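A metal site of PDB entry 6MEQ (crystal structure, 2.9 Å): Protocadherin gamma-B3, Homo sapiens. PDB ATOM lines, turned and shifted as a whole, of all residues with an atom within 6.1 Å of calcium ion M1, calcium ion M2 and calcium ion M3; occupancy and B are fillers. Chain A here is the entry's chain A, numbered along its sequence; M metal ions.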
ATOM      1  N   GLU A   9     -21.612  14.471  14.298  1.00  0.00           N
ATOM      2  CA  GLU A   9     -22.378  13.260  14.556  1.00  0.00           C
ATOM      3  C   GLU A   9     -23.512  13.544  15.531  1.00  0.00           C
ATOM      4  O   GLU A   9     -23.613  14.632  16.127  1.00  0.00           O
ATOM      5  CB  GLU A   9     -21.475  12.160  15.094  1.00  0.00           C
ATOM      6  CG  GLU A   9     -20.731  12.545  16.374  1.00  0.00           C
ATOM      7  CD  GLU A   9     -20.129  11.354  17.079  1.00  0.00           C
ATOM      8  OE1 GLU A   9     -20.619  10.225  16.861  1.00  0.00           O
ATOM      9  OE2 GLU A   9     -19.167  11.544  17.853  1.00  0.00           O
ATOM     10  N   GLU A  10     -24.380  12.544  15.697  1.00  0.00           N
ATOM     11  CA  GLU A  10     -25.488  12.591  16.655  1.00  0.00           C
ATOM     12  C   GLU A  10     -26.427  13.763  16.365  1.00  0.00           C
ATOM     13  O   GLU A  10     -26.962  14.398  17.277  1.00  0.00           O
ATOM     14  CB  GLU A  10     -24.984  12.649  18.092  1.00  0.00           C
ATOM     15  CG  GLU A  10     -24.061  11.492  18.479  1.00  0.00           C
ATOM     16  CD  GLU A  10     -24.786  10.160  18.520  1.00  0.00           C
ATOM     17  OE1 GLU A  10     -26.027  10.150  18.616  1.00  0.00           O
ATOM     18  OE2 GLU A  10     -24.101   9.121  18.456  1.00  0.00           O
ATOM     19  N   ARG A  59     -29.776   7.692  13.126  1.00  0.00           N
ATOM     20  CA  ARG A  59     -28.735   8.125  14.048  1.00  0.00           C
ATOM     21  C   ARG A  59     -27.366   7.762  13.505  1.00  0.00           C
ATOM     22  O   ARG A  59     -27.112   6.615  13.127  1.00  0.00           O
ATOM     23  CB  ARG A  59     -28.949   7.484  15.424  1.00  0.00           C
ATOM     24  CG  ARG A  59     -27.859   7.790  16.426  1.00  0.00           C
ATOM     25  CD  ARG A  59     -28.186   7.202  17.795  1.00  0.00           C
ATOM     26  NE  ARG A  59     -27.101   7.401  18.756  1.00  0.00           N
ATOM     27  CZ  ARG A  59     -26.141   6.514  18.990  1.00  0.00           C
ATOM     28  NH1 ARG A  59     -26.127   5.362  18.344  1.00  0.00           N
ATOM     29  NH2 ARG A  59     -25.199   6.784  19.890  1.00  0.00           N
ATOM     30  N   ILE A  60     -26.469   8.747  13.464  1.00  0.00           N
ATOM     31  CA  ILE A  60     -25.123   8.569  12.939  1.00  0.00           C
ATOM     32  C   ILE A  60     -24.174   8.569  14.140  1.00  0.00           C
ATOM     33  O   ILE A  60     -23.810   9.627  14.657  1.00  0.00           O
ATOM     34  CB  ILE A  60     -24.749   9.662  11.927  1.00  0.00           C
ATOM     35  CG1 ILE A  60     -25.746   9.674  10.775  1.00  0.00           C
ATOM     36  CG2 ILE A  60     -23.329   9.446  11.407  1.00  0.00           C
ATOM     37  CD1 ILE A  60     -25.460  10.729   9.728  1.00  0.00           C
ATOM     38  N   ASP A  61     -23.786   7.379  14.582  1.00  0.00           N
ATOM     39  CA  ASP A  61     -22.864   7.212  15.695  1.00  0.00           C
ATOM     40  C   ASP A  61     -21.478   6.920  15.131  1.00  0.00           C
ATOM     41  O   ASP A  61     -21.247   5.854  14.562  1.00  0.00           O
ATOM     42  CB  ASP A  61     -23.327   6.091  16.629  1.00  0.00           C
ATOM     43  CG  ASP A  61     -22.493   5.989  17.886  1.00  0.00           C
ATOM     44  OD1 ASP A  61     -21.670   6.905  18.146  1.00  0.00           O
ATOM     45  OD2 ASP A  61     -22.643   4.998  18.626  1.00  0.00           O
ATOM     46  N   ARG A  62     -20.555   7.872  15.293  1.00  0.00           N
ATOM     47  CA  ARG A  62     -19.217   7.699  14.734  1.00  0.00           C
ATOM     48  C   ARG A  62     -18.465   6.562  15.401  1.00  0.00           C
ATOM     49  O   ARG A  62     -17.631   5.904  14.757  1.00  0.00           O
ATOM     50  CB  ARG A  62     -18.424   9.005  14.862  1.00  0.00           C
ATOM     51  CG  ARG A  62     -17.146   9.030  14.047  1.00  0.00           C
ATOM     52  CD  ARG A  62     -16.105   9.934  14.669  1.00  0.00           C
ATOM     53  NE  ARG A  62     -15.743   9.492  16.008  1.00  0.00           N
ATOM     54  CZ  ARG A  62     -14.840   8.549  16.261  1.00  0.00           C
ATOM     55  NH1 ARG A  62     -14.201   7.960  15.260  1.00  0.00           N
ATOM     56  NH2 ARG A  62     -14.571   8.203  17.515  1.00  0.00           N
ATOM     57  N   GLU A  63     -18.730   6.302  16.684  1.00  0.00           N
ATOM     58  CA  GLU A  63     -18.043   5.210  17.368  1.00  0.00           C
ATOM     59  C   GLU A  63     -18.497   3.851  16.861  1.00  0.00           C
ATOM     60  O   GLU A  63     -17.721   2.888  16.919  1.00  0.00           O
ATOM     61  CB  GLU A  63     -18.267   5.321  18.888  1.00  0.00           C
ATOM     62  CG  GLU A  63     -17.427   6.377  19.575  1.00  0.00           C
ATOM     63  CD  GLU A  63     -17.834   7.789  19.208  1.00  0.00           C
ATOM     64  OE1 GLU A  63     -19.057   8.048  19.094  1.00  0.00           O
ATOM     65  OE2 GLU A  63     -16.932   8.644  19.028  1.00  0.00           O
ATOM     66  N   ASP A  95     -16.343  14.295  14.853  1.00  0.00           N
ATOM     67  CA  ASP A  95     -16.431  13.649  16.157  1.00  0.00           C
ATOM     68  C   ASP A  95     -16.726  14.673  17.244  1.00  0.00           C
ATOM     69  O   ASP A  95     -16.123  15.753  17.280  1.00  0.00           O
ATOM     70  CB  ASP A  95     -15.135  12.901  16.476  1.00  0.00           C
ATOM     71  CG  ASP A  95     -15.158  12.287  17.862  1.00  0.00           C
ATOM     72  OD1 ASP A  95     -15.969  11.374  18.098  1.00  0.00           O
ATOM     73  OD2 ASP A  95     -14.353  12.721  18.714  1.00  0.00           O
ATOM     74  N   ILE A  96     -17.653  14.327  18.131  1.00  0.00           N
ATOM     75  CA  ILE A  96     -17.982  15.147  19.285  1.00  0.00           C
ATOM     76  C   ILE A  96     -17.626  14.367  20.547  1.00  0.00           C
ATOM     77  O   ILE A  96     -17.546  13.138  20.543  1.00  0.00           O
ATOM     78  CB  ILE A  96     -19.465  15.566  19.305  1.00  0.00           C
ATOM     79  CG1 ILE A  96     -20.364  14.346  19.499  1.00  0.00           C
ATOM     80  CG2 ILE A  96     -19.828  16.314  18.037  1.00  0.00           C
ATOM     81  CD1 ILE A  96     -21.846  14.681  19.569  1.00  0.00           C
ATOM     82  N   ASN A  97     -17.402  15.109  21.633  1.00  0.00           N
ATOM     83  CA  ASN A  97     -17.031  14.513  22.912  1.00  0.00           C
ATOM     84  C   ASN A  97     -18.313  14.136  23.654  1.00  0.00           C
ATOM     85  O   ASN A  97     -18.793  14.842  24.543  1.00  0.00           O
ATOM     86  CB  ASN A  97     -16.162  15.459  23.725  1.00  0.00           C
ATOM     87  CG  ASN A  97     -15.648  14.825  24.994  1.00  0.00           C
ATOM     88  OD1 ASN A  97     -15.549  13.612  25.097  1.00  0.00           O
ATOM     89  ND2 ASN A  97     -15.314  15.658  25.983  1.00  0.00           N
ATOM     90  N   ASP A  98     -18.869  12.985  23.278  1.00  0.00           N
ATOM     91  CA  ASP A  98     -20.095  12.479  23.882  1.00  0.00           C
ATOM     92  C   ASP A  98     -19.881  11.154  24.605  1.00  0.00           C
ATOM     93  O   ASP A  98     -20.846  10.457  24.925  1.00  0.00           O
ATOM     94  CB  ASP A  98     -21.195  12.334  22.823  1.00  0.00           C
ATOM     95  CG  ASP A  98     -20.765  11.481  21.648  1.00  0.00           C
ATOM     96  OD1 ASP A  98     -19.584  11.109  21.575  1.00  0.00           O
ATOM     97  OD2 ASP A  98     -21.629  11.184  20.794  1.00  0.00           O
ATOM     98  N   ASN A  99     -18.623  10.793  24.875  1.00  0.00           N
ATOM     99  CA  ASN A  99     -18.315   9.548  25.561  1.00  0.00           C
ATOM    100  C   ASN A  99     -17.232   9.776  26.610  1.00  0.00           C
ATOM    101  O   ASN A  99     -16.117  10.187  26.261  1.00  0.00           O
ATOM    102  CB  ASN A  99     -17.872   8.475  24.562  1.00  0.00           C
ATOM    103  CG  ASN A  99     -19.016   8.004  23.676  1.00  0.00           C
ATOM    104  OD1 ASN A  99     -18.982   8.182  22.459  1.00  0.00           O
ATOM    105  ND2 ASN A  99     -20.026   7.388  24.283  1.00  0.00           N
ATOM    106  N   PRO A 100     -17.516   9.517  27.878  1.00  0.00           N
ATOM    107  CA  PRO A 100     -16.509   9.724  28.923  1.00  0.00           C
ATOM    108  C   PRO A 100     -15.488   8.604  28.927  1.00  0.00           C
ATOM    109  O   PRO A 100     -15.784   7.489  28.460  1.00  0.00           O
ATOM    110  CB  PRO A 100     -17.348   9.723  30.209  1.00  0.00           C
ATOM    111  CG  PRO A 100     -18.500   8.847  29.891  1.00  0.00           C
ATOM    112  CD  PRO A 100     -18.806   9.076  28.432  1.00  0.00           C
ATOM    113  N   PRO A 101     -14.286   8.860  29.421  1.00  0.00           N
ATOM    114  CA  PRO A 101     -13.298   7.781  29.546  1.00  0.00           C
ATOM    115  C   PRO A 101     -13.706   6.799  30.641  1.00  0.00           C
ATOM    116  O   PRO A 101     -14.606   7.048  31.440  1.00  0.00           O
ATOM    117  CB  PRO A 101     -12.013   8.519  29.905  1.00  0.00           C
ATOM    118  CG  PRO A 101     -12.472   9.781  30.555  1.00  0.00           C
ATOM    119  CD  PRO A 101     -13.744  10.157  29.858  1.00  0.00           C
ATOM    120  N   ASP A 129     -10.951   5.580  25.795  1.00  0.00           N
ATOM    121  CA  ASP A 129     -12.041   6.437  25.356  1.00  0.00           C
ATOM    122  C   ASP A 129     -12.409   6.091  23.919  1.00  0.00           C
ATOM    123  O   ASP A 129     -11.545   6.117  23.033  1.00  0.00           O
ATOM    124  CB  ASP A 129     -11.628   7.904  25.472  1.00  0.00           C
ATOM    125  CG  ASP A 129     -12.821   8.850  25.452  1.00  0.00           C
ATOM    126  OD1 ASP A 129     -13.720   8.674  24.605  1.00  0.00           O
ATOM    127  OD2 ASP A 129     -12.854   9.780  26.288  1.00  0.00           O
ATOM    128  N   PRO A 130     -13.675   5.755  23.647  1.00  0.00           N
ATOM    129  CA  PRO A 130     -14.060   5.400  22.271  1.00  0.00           C
ATOM    130  C   PRO A 130     -14.004   6.566  21.292  1.00  0.00           C
ATOM    131  O   PRO A 130     -14.128   6.343  20.089  1.00  0.00           O
ATOM    132  CB  PRO A 130     -15.499   4.887  22.436  1.00  0.00           C
ATOM    133  CG  PRO A 130     -15.985   5.527  23.684  1.00  0.00           C
ATOM    134  CD  PRO A 130     -14.795   5.628  24.597  1.00  0.00           C
ATOM    135  N   ASP A 131     -13.825   7.797  21.769  1.00  0.00           N
ATOM    136  CA  ASP A 131     -13.713   8.953  20.890  1.00  0.00           C
ATOM    137  C   ASP A 131     -12.322   8.982  20.248  1.00  0.00           C
ATOM    138  O   ASP A 131     -11.470   8.134  20.500  1.00  0.00           O
ATOM    139  CB  ASP A 131     -14.002  10.238  21.661  1.00  0.00           C
ATOM    140  CG  ASP A 131     -15.402  10.274  22.244  1.00  0.00           C
ATOM    141  OD1 ASP A 131     -16.317   9.707  21.614  1.00  0.00           O
ATOM    142  OD2 ASP A 131     -15.579  10.866  23.327  1.00  0.00           O
ATOM    143  N   VAL A 132     -12.100   9.980  19.397  1.00  0.00           N
ATOM    144  CA  VAL A 132     -10.825  10.171  18.713  1.00  0.00           C
ATOM    145  C   VAL A 132     -10.421  11.633  18.840  1.00  0.00           C
ATOM    146  O   VAL A 132     -11.192  12.481  19.291  1.00  0.00           O
ATOM    147  CB  VAL A 132     -10.887   9.748  17.232  1.00  0.00           C
ATOM    148  CG1 VAL A 132     -11.159   8.257  17.102  1.00  0.00           C
ATOM    149  CG2 VAL A 132     -11.936  10.564  16.486  1.00  0.00           C
ATOM    150  N   ASN A 135     -10.762  14.602  21.859  1.00  0.00           N
ATOM    151  CA  ASN A 135     -11.833  14.073  22.707  1.00  0.00           C
ATOM    152  C   ASN A 135     -11.414  12.816  23.444  1.00  0.00           C
ATOM    153  O   ASN A 135     -12.049  12.457  24.436  1.00  0.00           O
ATOM    154  CB  ASN A 135     -13.080  13.797  21.870  1.00  0.00           C
ATOM    155  CG  ASN A 135     -13.580  15.025  21.129  1.00  0.00           C
ATOM    156  OD1 ASN A 135     -13.388  16.150  21.590  1.00  0.00           O
ATOM    157  ND2 ASN A 135     -14.213  14.813  19.988  1.00  0.00           N
ATOM    158  N   SER A 136     -10.351  12.144  22.996  1.00  0.00           N
ATOM    159  CA  SER A 136      -9.827  10.969  23.668  1.00  0.00           C
ATOM    160  C   SER A 136      -8.473  11.214  24.339  1.00  0.00           C
ATOM    161  O   SER A 136      -7.982  10.328  25.036  1.00  0.00           O
ATOM    162  CB  SER A 136      -9.692   9.804  22.687  1.00  0.00           C
ATOM    163  OG  SER A 136      -8.798  10.117  21.631  1.00  0.00           O
ATOM    164  N   GLN A 138      -6.320  11.948  27.047  1.00  0.00           N
ATOM    165  CA  GLN A 138      -6.580  11.935  28.478  1.00  0.00           C
ATOM    166  C   GLN A 138      -5.512  12.729  29.235  1.00  0.00           C
ATOM    167  O   GLN A 138      -4.367  12.839  28.810  1.00  0.00           O
ATOM    168  CB  GLN A 138      -6.613  10.503  29.005  1.00  0.00           C
ATOM    169  CG  GLN A 138      -7.637   9.620  28.309  1.00  0.00           C
ATOM    170  CD  GLN A 138      -9.054  10.132  28.451  1.00  0.00           C
ATOM    171  OE1 GLN A 138      -9.412  10.735  29.466  1.00  0.00           O
ATOM    172  NE2 GLN A 138      -9.867   9.890  27.430  1.00  0.00           N
ATOM    173  N   ASP A 186     -10.470  14.015  29.815  1.00  0.00           N
ATOM    174  CA  ASP A 186     -10.167  14.158  28.397  1.00  0.00           C
ATOM    175  C   ASP A 186     -10.108  15.638  28.015  1.00  0.00           C
ATOM    176  O   ASP A 186     -10.494  16.529  28.782  1.00  0.00           O
ATOM    177  CB  ASP A 186     -11.199  13.419  27.543  1.00  0.00           C
ATOM    178  CG  ASP A 186     -12.620  13.890  27.788  1.00  0.00           C
ATOM    179  OD1 ASP A 186     -12.825  14.804  28.616  1.00  0.00           O
ATOM    180  OD2 ASP A 186     -13.543  13.340  27.141  1.00  0.00           O
ATOM    181  N   ARG A 192     -15.365  15.403  30.115  1.00  0.00           N
ATOM    182  CA  ARG A 192     -15.872  14.243  30.835  1.00  0.00           C
ATOM    183  C   ARG A 192     -14.720  13.523  31.512  1.00  0.00           C
ATOM    184  O   ARG A 192     -13.618  13.438  30.961  1.00  0.00           O
ATOM    185  CB  ARG A 192     -16.614  13.302  29.895  1.00  0.00           C
ATOM    186  CG  ARG A 192     -17.991  13.810  29.470  1.00  0.00           C
ATOM    187  CD  ARG A 192     -18.654  12.850  28.490  1.00  0.00           C
ATOM    188  NE  ARG A 192     -20.069  13.152  28.299  1.00  0.00           N
ATOM    189  CZ  ARG A 192     -20.527  14.056  27.448  1.00  0.00           C
ATOM    190  NH1 ARG A 192     -19.683  14.756  26.698  1.00  0.00           N
ATOM    191  NH2 ARG A 192     -21.833  14.264  27.335  1.00  0.00           N
HETATM  192 CA    CA M   1     -17.811  10.766  19.792  1.00  0.00          CA
HETATM  193 CA    CA M   2     -14.202  11.537  25.226  1.00  0.00          CA
HETATM  194 CA    CA M   3     -21.343   9.051  19.391  1.00  0.00          CA
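The side-chain carboxylate (OD2) of Asp 129 sits close to the side-chain amide nitrogen (NE2) of Gln 138 (3.2 Å). The side-chain carboxylate (OE1) of Glu 63 sits close to the side-chain amide oxygen (OD1) of Asn 99 (3.4 Å). The side-chain amide oxygen (OD1) of Asn 99 lies close to the side-chain carboxylate (OD1) of Asp 98 (3.1 Å). The guanidinium group (NH2) of Arg 59 lies within salt-bridge range of the side-chain carboxylate (OE2) of Glu 10. The side-chain carboxylate (OE1) of Glu 9 sits close to the backbone NH (N) of Arg 62 (2.8 Å). N of Glu 10 lies within hydrogen-bond range of O of Ile 60 (3.1 Å). The side-chain carboxylate (OD1) of Asp 186 sits at hydrogen-bond distance from the backbone NH (N) of Arg 192 (3.0 Å). N of Asp 186 sits at hydrogen-bond distance from OE1 of Gln 138 (3.5 Å).
Calcium ion M3 is bound by the side-chain carboxylate of Asp 61 (2.5 Å), the side-chain carboxylate of Glu 63 (2.5 Å), the side-chain carboxylate of Asp 98 (2.6 Å) and the side-chain carboxylate of Glu 9 (2.9 Å). Slightly farther from calcium ion M3 lies the side-chain carboxylate (OE2) of Glu 10 (2.9 Å).
Calcium ion M1 is bound by OE2 of Glu 63 (2.4 Å), OE2 of Glu 9 (2.5 Å), O of Ile 96 (2.5 Å), OD1 of Asp 98 (2.5 Å), OD1 of Asp 95 (2.6 Å) and OD1 of Asp 131 (2.6 Å). Calcium ion M1 has six donor atoms within binding distance. Slightly farther from calcium ion M1 lies OE1 of Glu 63 (3.1 Å).
Of the 23 residues printed, 6 come within 4 Å of calcium ion M2. The nearest printed residue that does not touch calcium ion M2 is Ser 136 (4.5 Å).
Calcium ion M2 is bound by the side-chain carboxylate of Asp 131 (2.4 Å), the side-chain carboxylate of Asp 129 (2.5 Å), the backbone carbonyl oxygen of Asn 135 (2.5 Å), the side-chain amide oxygen of Asn 97 (2.5 Å), the backbone carbonyl oxygen of Asn 99 (2.6 Å) and the side-chain carboxylate of Asp 186 (2.7 Å). Calcium ion M2 has six donor atoms within binding distance. Slightly farther from calcium ion M2 lies the side-chain carboxylate (OD1) of Asp 129 (3.0 Å).
Six residues have an atom within 4 Å of calcium ion M3: Glu 9, Glu 10, Asp 61, Glu 63, Asp 98 and Asn 99.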
